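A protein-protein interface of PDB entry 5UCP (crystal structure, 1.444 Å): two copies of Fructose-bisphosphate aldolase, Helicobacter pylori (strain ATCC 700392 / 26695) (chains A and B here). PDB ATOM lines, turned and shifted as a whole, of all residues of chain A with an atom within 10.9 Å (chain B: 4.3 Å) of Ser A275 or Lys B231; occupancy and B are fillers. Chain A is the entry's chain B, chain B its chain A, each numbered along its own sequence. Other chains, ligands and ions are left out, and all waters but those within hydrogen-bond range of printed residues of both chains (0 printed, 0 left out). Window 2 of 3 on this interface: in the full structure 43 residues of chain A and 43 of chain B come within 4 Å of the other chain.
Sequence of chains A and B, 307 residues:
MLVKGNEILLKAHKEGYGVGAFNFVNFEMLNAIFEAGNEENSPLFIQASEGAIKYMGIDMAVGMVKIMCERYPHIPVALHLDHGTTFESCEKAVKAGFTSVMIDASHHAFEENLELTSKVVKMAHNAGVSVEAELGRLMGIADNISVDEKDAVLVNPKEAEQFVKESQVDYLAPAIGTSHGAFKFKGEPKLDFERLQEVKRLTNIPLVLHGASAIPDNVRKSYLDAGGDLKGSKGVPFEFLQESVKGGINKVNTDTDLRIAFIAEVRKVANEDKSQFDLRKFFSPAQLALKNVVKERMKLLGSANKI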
ATOM      1  N   LYS A 268      19.097 -19.145  -9.391  1.00  0.00           N
ATOM      2  CA  LYS A 268      18.272 -18.716 -10.514  1.00  0.00           C
ATOM      3  C   LYS A 268      19.034 -17.756 -11.420  1.00  0.00           C
ATOM      4  O   LYS A 268      19.039 -17.914 -12.648  1.00  0.00           O
ATOM      5  CB  LYS A 268      17.001 -18.066  -9.970  1.00  0.00           C
ATOM      6  CG  LYS A 268      16.041 -17.553 -11.016  1.00  0.00           C
ATOM      7  CD  LYS A 268      14.674 -17.288 -10.397  1.00  0.00           C
ATOM      8  CE  LYS A 268      13.705 -16.691 -11.404  1.00  0.00           C
ATOM      9  NZ  LYS A 268      14.122 -15.330 -11.836  1.00  0.00           N
ATOM     10  N   VAL A 269      19.697 -16.757 -10.834  1.00  0.00           N
ATOM     11  CA  VAL A 269      20.471 -15.817 -11.644  1.00  0.00           C
ATOM     12  C   VAL A 269      21.561 -16.549 -12.411  1.00  0.00           C
ATOM     13  O   VAL A 269      21.778 -16.300 -13.604  1.00  0.00           O
ATOM     14  CB  VAL A 269      21.040 -14.683 -10.770  1.00  0.00           C
ATOM     15  CG1 VAL A 269      22.016 -13.825 -11.568  1.00  0.00           C
ATOM     16  CG2 VAL A 269      19.915 -13.827 -10.224  1.00  0.00           C
ATOM     17  N   ALA A 270      22.262 -17.467 -11.744  1.00  0.00           N
ATOM     18  CA  ALA A 270      23.330 -18.201 -12.415  1.00  0.00           C
ATOM     19  C   ALA A 270      22.788 -18.998 -13.588  1.00  0.00           C
ATOM     20  O   ALA A 270      23.442 -19.096 -14.633  1.00  0.00           O
ATOM     21  CB  ALA A 270      24.033 -19.131 -11.426  1.00  0.00           C
ATOM     22  N   ASN A 271      21.592 -19.571 -13.433  1.00  0.00           N
ATOM     23  CA  ASN A 271      21.008 -20.416 -14.474  1.00  0.00           C
ATOM     24  C   ASN A 271      20.539 -19.598 -15.670  1.00  0.00           C
ATOM     25  O   ASN A 271      20.645 -20.049 -16.816  1.00  0.00           O
ATOM     26  CB  ASN A 271      19.808 -21.172 -13.910  1.00  0.00           C
ATOM     27  CG  ASN A 271      20.192 -22.217 -12.891  1.00  0.00           C
ATOM     28  OD1 ASN A 271      21.339 -22.655 -12.823  1.00  0.00           O
ATOM     29  ND2 ASN A 271      19.216 -22.636 -12.093  1.00  0.00           N
ATOM     30  N   GLU A 272      19.981 -18.415 -15.426  1.00  0.00           N
ATOM     31  CA  GLU A 272      19.296 -17.664 -16.467  1.00  0.00           C
ATOM     32  C   GLU A 272      20.203 -16.735 -17.260  1.00  0.00           C
ATOM     33  O   GLU A 272      19.762 -16.220 -18.291  1.00  0.00           O
ATOM     34  CB  GLU A 272      18.151 -16.851 -15.868  1.00  0.00           C
ATOM     35  CG  GLU A 272      17.040 -17.718 -15.288  1.00  0.00           C
ATOM     36  CD  GLU A 272      15.834 -16.916 -14.847  1.00  0.00           C
ATOM     37  OE1 GLU A 272      15.968 -15.692 -14.625  1.00  0.00           O
ATOM     38  OE2 GLU A 272      14.746 -17.514 -14.724  1.00  0.00           O
ATOM     39  N   ASP A 273      21.441 -16.496 -16.813  1.00  0.00           N
ATOM     40  CA  ASP A 273      22.373 -15.646 -17.563  1.00  0.00           C
ATOM     41  C   ASP A 273      23.800 -16.103 -17.257  1.00  0.00           C
ATOM     42  O   ASP A 273      24.386 -15.692 -16.250  1.00  0.00           O
ATOM     43  CB  ASP A 273      22.177 -14.174 -17.226  1.00  0.00           C
ATOM     44  CG  ASP A 273      23.032 -13.261 -18.096  1.00  0.00           C
ATOM     45  OD1 ASP A 273      23.878 -13.783 -18.852  1.00  0.00           O
ATOM     46  OD2 ASP A 273      22.854 -12.026 -18.034  1.00  0.00           O
ATOM     47  N   LYS A 274      24.362 -16.923 -18.148  1.00  0.00           N
ATOM     48  CA  LYS A 274      25.715 -17.435 -17.954  1.00  0.00           C
ATOM     49  C   LYS A 274      26.781 -16.347 -18.040  1.00  0.00           C
ATOM     50  O   LYS A 274      27.916 -16.577 -17.608  1.00  0.00           O
ATOM     51  CB  LYS A 274      26.004 -18.530 -18.983  1.00  0.00           C
ATOM     52  CG  LYS A 274      25.004 -19.675 -18.957  1.00  0.00           C
ATOM     53  CD  LYS A 274      24.979 -20.342 -17.588  1.00  0.00           C
ATOM     54  CE  LYS A 274      24.032 -21.512 -17.513  1.00  0.00           C
ATOM     55  NZ  LYS A 274      24.131 -22.129 -16.166  1.00  0.00           N
ATOM     56  N   SER A 275      26.456 -15.178 -18.578  1.00  0.00           N
ATOM     57  CA  SER A 275      27.426 -14.101 -18.672  1.00  0.00           C
ATOM     58  C   SER A 275      27.375 -13.150 -17.483  1.00  0.00           C
ATOM     59  O   SER A 275      28.152 -12.194 -17.448  1.00  0.00           O
ATOM     60  CB  SER A 275      27.233 -13.311 -19.972  1.00  0.00           C
ATOM     61  OG  SER A 275      26.086 -12.482 -19.892  1.00  0.00           O
ATOM     62  N   GLN A 276      26.506 -13.392 -16.508  1.00  0.00           N
ATOM     63  CA  GLN A 276      26.320 -12.453 -15.410  1.00  0.00           C
ATOM     64  C   GLN A 276      27.365 -12.705 -14.328  1.00  0.00           C
ATOM     65  O   GLN A 276      27.429 -13.804 -13.760  1.00  0.00           O
ATOM     66  CB  GLN A 276      24.917 -12.625 -14.834  1.00  0.00           C
ATOM     67  CG  GLN A 276      24.574 -11.656 -13.695  1.00  0.00           C
ATOM     68  CD  GLN A 276      24.615 -10.205 -14.132  1.00  0.00           C
ATOM     69  OE1 GLN A 276      25.618  -9.511 -13.945  1.00  0.00           O
ATOM     70  NE2 GLN A 276      23.516  -9.734 -14.714  1.00  0.00           N
ATOM     71  N   PHE A 277      28.168 -11.685 -14.020  1.00  0.00           N
ATOM     72  CA  PHE A 277      29.096 -11.766 -12.896  1.00  0.00           C
ATOM     73  C   PHE A 277      29.090 -10.508 -12.026  1.00  0.00           C
ATOM     74  O   PHE A 277      30.008 -10.316 -11.224  1.00  0.00           O
ATOM     75  CB  PHE A 277      30.515 -12.139 -13.334  1.00  0.00           C
ATOM     76  CG  PHE A 277      31.047 -11.314 -14.472  1.00  0.00           C
ATOM     77  CD1 PHE A 277      31.529 -10.040 -14.252  1.00  0.00           C
ATOM     78  CD2 PHE A 277      31.086 -11.825 -15.756  1.00  0.00           C
ATOM     79  CE1 PHE A 277      32.032  -9.284 -15.295  1.00  0.00           C
ATOM     80  CE2 PHE A 277      31.582 -11.070 -16.799  1.00  0.00           C
ATOM     81  CZ  PHE A 277      32.051  -9.803 -16.564  1.00  0.00           C
ATOM     82  N   ASP A 278      28.075  -9.657 -12.147  1.00  0.00           N
ATOM     83  CA  ASP A 278      27.886  -8.562 -11.198  1.00  0.00           C
ATOM     84  C   ASP A 278      27.281  -9.143  -9.931  1.00  0.00           C
ATOM     85  O   ASP A 278      26.147  -9.631  -9.945  1.00  0.00           O
ATOM     86  CB  ASP A 278      26.966  -7.504 -11.796  1.00  0.00           C
ATOM     87  CG  ASP A 278      26.811  -6.274 -10.908  1.00  0.00           C
ATOM     88  OD1 ASP A 278      27.098  -6.338  -9.697  1.00  0.00           O
ATOM     89  OD2 ASP A 278      26.376  -5.231 -11.430  1.00  0.00           O
ATOM     90  N   LEU A 279      28.036  -9.080  -8.832  1.00  0.00           N
ATOM     91  CA  LEU A 279      27.563  -9.658  -7.576  1.00  0.00           C
ATOM     92  C   LEU A 279      26.206  -9.092  -7.181  1.00  0.00           C
ATOM     93  O   LEU A 279      25.361  -9.814  -6.633  1.00  0.00           O
ATOM     94  CB  LEU A 279      28.587  -9.418  -6.466  1.00  0.00           C
ATOM     95  CG  LEU A 279      29.752 -10.411  -6.321  1.00  0.00           C
ATOM     96  CD1 LEU A 279      30.709 -10.360  -7.477  1.00  0.00           C
ATOM     97  CD2 LEU A 279      30.514 -10.167  -5.026  1.00  0.00           C
ATOM     98  N   LYS A 281      23.724  -8.221  -9.030  1.00  0.00           N
ATOM     99  CA  LYS A 281      22.631  -8.834  -9.772  1.00  0.00           C
ATOM    100  C   LYS A 281      22.243 -10.193  -9.203  1.00  0.00           C
ATOM    101  O   LYS A 281      21.107 -10.633  -9.392  1.00  0.00           O
ATOM    102  CB  LYS A 281      23.011  -8.985 -11.236  1.00  0.00           C
ATOM    103  CG  LYS A 281      23.212  -7.665 -11.973  1.00  0.00           C
ATOM    104  CD  LYS A 281      21.909  -6.945 -12.221  1.00  0.00           C
ATOM    105  CE  LYS A 281      22.143  -5.659 -13.001  1.00  0.00           C
ATOM    106  NZ  LYS A 281      20.879  -4.923 -13.253  1.00  0.00           N
ATOM    107  N   PHE A 282      23.170 -10.882  -8.532  1.00  0.00           N
ATOM    108  CA  PHE A 282      22.836 -12.097  -7.801  1.00  0.00           C
ATOM    109  C   PHE A 282      22.190 -11.779  -6.460  1.00  0.00           C
ATOM    110  O   PHE A 282      21.213 -12.429  -6.065  1.00  0.00           O
ATOM    111  CB  PHE A 282      24.100 -12.919  -7.544  1.00  0.00           C
ATOM    112  CG  PHE A 282      24.681 -13.560  -8.770  1.00  0.00           C
ATOM    113  CD1 PHE A 282      25.547 -12.863  -9.605  1.00  0.00           C
ATOM    114  CD2 PHE A 282      24.369 -14.865  -9.085  1.00  0.00           C
ATOM    115  CE1 PHE A 282      26.086 -13.467 -10.728  1.00  0.00           C
ATOM    116  CE2 PHE A 282      24.901 -15.466 -10.205  1.00  0.00           C
ATOM    117  CZ  PHE A 282      25.763 -14.762 -11.027  1.00  0.00           C
ATOM    118  N   PHE B 183      35.095  -6.533 -22.103  1.00  0.00           N
ATOM    119  CA  PHE B 183      35.200  -6.454 -23.559  1.00  0.00           C
ATOM    120  C   PHE B 183      35.855  -5.122 -23.896  1.00  0.00           C
ATOM    121  O   PHE B 183      35.180  -4.140 -24.214  1.00  0.00           O
ATOM    122  CB  PHE B 183      33.808  -6.591 -24.160  1.00  0.00           C
ATOM    123  CG  PHE B 183      32.956  -7.619 -23.466  1.00  0.00           C
ATOM    124  CD1 PHE B 183      33.133  -8.971 -23.715  1.00  0.00           C
ATOM    125  CD2 PHE B 183      31.990  -7.234 -22.551  1.00  0.00           C
ATOM    126  CE1 PHE B 183      32.357  -9.917 -23.071  1.00  0.00           C
ATOM    127  CE2 PHE B 183      31.210  -8.177 -21.906  1.00  0.00           C
ATOM    128  CZ  PHE B 183      31.393  -9.520 -22.167  1.00  0.00           C
ATOM    129  N   TYR B 223      35.917 -19.699 -14.854  1.00  0.00           N
ATOM    130  CA  TYR B 223      34.576 -19.232 -15.178  1.00  0.00           C
ATOM    131  C   TYR B 223      33.912 -20.147 -16.201  1.00  0.00           C
ATOM    132  O   TYR B 223      32.751 -20.537 -16.041  1.00  0.00           O
ATOM    133  CB  TYR B 223      34.625 -17.787 -15.686  1.00  0.00           C
ATOM    134  CG  TYR B 223      33.275 -17.120 -15.660  1.00  0.00           C
ATOM    135  CD1 TYR B 223      32.734 -16.663 -14.464  1.00  0.00           C
ATOM    136  CD2 TYR B 223      32.535 -16.951 -16.820  1.00  0.00           C
ATOM    137  CE1 TYR B 223      31.496 -16.059 -14.432  1.00  0.00           C
ATOM    138  CE2 TYR B 223      31.294 -16.337 -16.795  1.00  0.00           C
ATOM    139  CZ  TYR B 223      30.774 -15.902 -15.589  1.00  0.00           C
ATOM    140  OH  TYR B 223      29.540 -15.299 -15.524  1.00  0.00           O
ATOM    141  N   ASP B 229      29.793 -17.908 -19.470  1.00  0.00           N
ATOM    142  CA  ASP B 229      30.018 -17.432 -20.828  1.00  0.00           C
ATOM    143  C   ASP B 229      30.685 -16.070 -20.748  1.00  0.00           C
ATOM    144  O   ASP B 229      30.121 -15.134 -20.175  1.00  0.00           O
ATOM    145  CB  ASP B 229      28.691 -17.304 -21.572  1.00  0.00           C
ATOM    146  CG  ASP B 229      28.863 -16.799 -22.985  1.00  0.00           C
ATOM    147  OD1 ASP B 229      30.009 -16.790 -23.477  1.00  0.00           O
ATOM    148  OD2 ASP B 229      27.850 -16.406 -23.597  1.00  0.00           O
ATOM    149  N   LEU B 230      31.880 -15.966 -21.313  1.00  0.00           N
ATOM    150  CA  LEU B 230      32.596 -14.701 -21.425  1.00  0.00           C
ATOM    151  C   LEU B 230      32.552 -14.315 -22.901  1.00  0.00           C
ATOM    152  O   LEU B 230      33.408 -14.709 -23.694  1.00  0.00           O
ATOM    153  CB  LEU B 230      34.017 -14.838 -20.889  1.00  0.00           C
ATOM    154  CG  LEU B 230      34.110 -14.965 -19.365  1.00  0.00           C
ATOM    155  CD1 LEU B 230      35.504 -15.401 -18.931  1.00  0.00           C
ATOM    156  CD2 LEU B 230      33.722 -13.662 -18.682  1.00  0.00           C
ATOM    157  N   LYS B 231      31.533 -13.537 -23.254  1.00  0.00           N
ATOM    158  CA  LYS B 231      31.188 -13.234 -24.638  1.00  0.00           C
ATOM    159  C   LYS B 231      32.329 -12.578 -25.416  1.00  0.00           C
ATOM    160  O   LYS B 231      32.318 -11.360 -25.628  1.00  0.00           O
ATOM    161  CB  LYS B 231      29.960 -12.319 -24.638  1.00  0.00           C
ATOM    162  CG  LYS B 231      28.726 -12.940 -23.985  1.00  0.00           C
ATOM    163  CD  LYS B 231      27.658 -11.897 -23.665  1.00  0.00           C
ATOM    164  CE  LYS B 231      26.284 -12.541 -23.519  1.00  0.00           C
ATOM    165  NZ  LYS B 231      25.328 -11.705 -22.735  1.00  0.00           N
ATOM    166  N   GLY B 232      33.308 -13.367 -25.861  1.00  0.00           N
ATOM    167  CA  GLY B 232      34.413 -12.813 -26.631  1.00  0.00           C
ATOM    168  C   GLY B 232      35.224 -11.778 -25.884  1.00  0.00           C
ATOM    169  O   GLY B 232      35.745 -10.837 -26.495  1.00  0.00           O
ATOM    170  N   SER B 233      35.358 -11.936 -24.574  1.00  0.00           N
ATOM    171  CA  SER B 233      36.011 -10.949 -23.734  1.00  0.00           C
ATOM    172  C   SER B 233      37.511 -10.890 -24.014  1.00  0.00           C
ATOM    173  O   SER B 233      38.120 -11.835 -24.525  1.00  0.00           O
ATOM    174  CB  SER B 233      35.790 -11.306 -22.264  1.00  0.00           C
ATOM    175  OG  SER B 233      36.244 -12.623 -22.006  1.00  0.00           O
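No position is printed for both chains.
The side-chain hydroxyl of Tyr B223 is in hydrogen-bond range of the backbone carbonyl oxygen of Lys A274.
OH of Tyr B223 lies within hydrogen-bond range of O of Gln A276, 3.1 Å away.
The backbone NH of Asp B229 sits at hydrogen-bond distance from the backbone carbonyl oxygen of Lys A274, 3.0 Å away.
OG of Ser A275 sits at hydrogen-bond distance from NZ of Lys B231 (3.0 Å).
Among the printed residues, pairs that only touch across the chains: Ser A275 with Asp B229, Ser A275 with Tyr B223, Phe A277 with Tyr B223 and Phe A277 with Leu B230.
Of the printed residues of chain B, Lys A274 touches Tyr B223 (2.9 Å) and Asp B229 (3.0 Å).
Ser A275 touches just these residues of chain B: Tyr B223, Asp B229 and Lys B231.
Of the printed residues of chain B, Phe A277 touches Tyr B223 and Leu B230.
Of the printed residues of chain A, Tyr B223 touches Lys A274, Ser A275, Gln A276 and Phe A277.
Of chain A, only Lys A274 (3.0 Å) and Ser A275 (3.3 Å) come within 4 Å of Asp B229.
Of the printed residues of chain A, Lys B231 touches Ser A275.
No residue of chain A comes within 4 Å of Gly B232.
The nearest residue of chain A that does not touch Lys B231 is Asp A273 (4.6 Å).
The nearest printed residue of chain B that does not touch Lys A274 is Leu B230 (5.5 Å).
Printed residues of chain A that touch a printed residue of chain B: Lys A274, Ser A275, Gln A276 and Phe A277.
Among the printed residues, no Asp or Glu carboxylate lies within 4 Å of a Lys or Arg side-chain nitrogen of the other chain.
The backbone carbonyl oxygen (O) of Ala A270 is in hydrogen-bond range of the side-chain amino group (NZ) of Lys A274, 3.5 Å away.
The side-chain hydroxyl (OG) of Ser A275 lies within hydrogen-bond range of the side-chain carboxylate (OD1) of Asp A273 (2.8 Å).
The side-chain amide oxygen (OE1) of Gln A276 sits at hydrogen-bond distance from the backbone NH (N) of Asp A278, 3.0 Å away.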
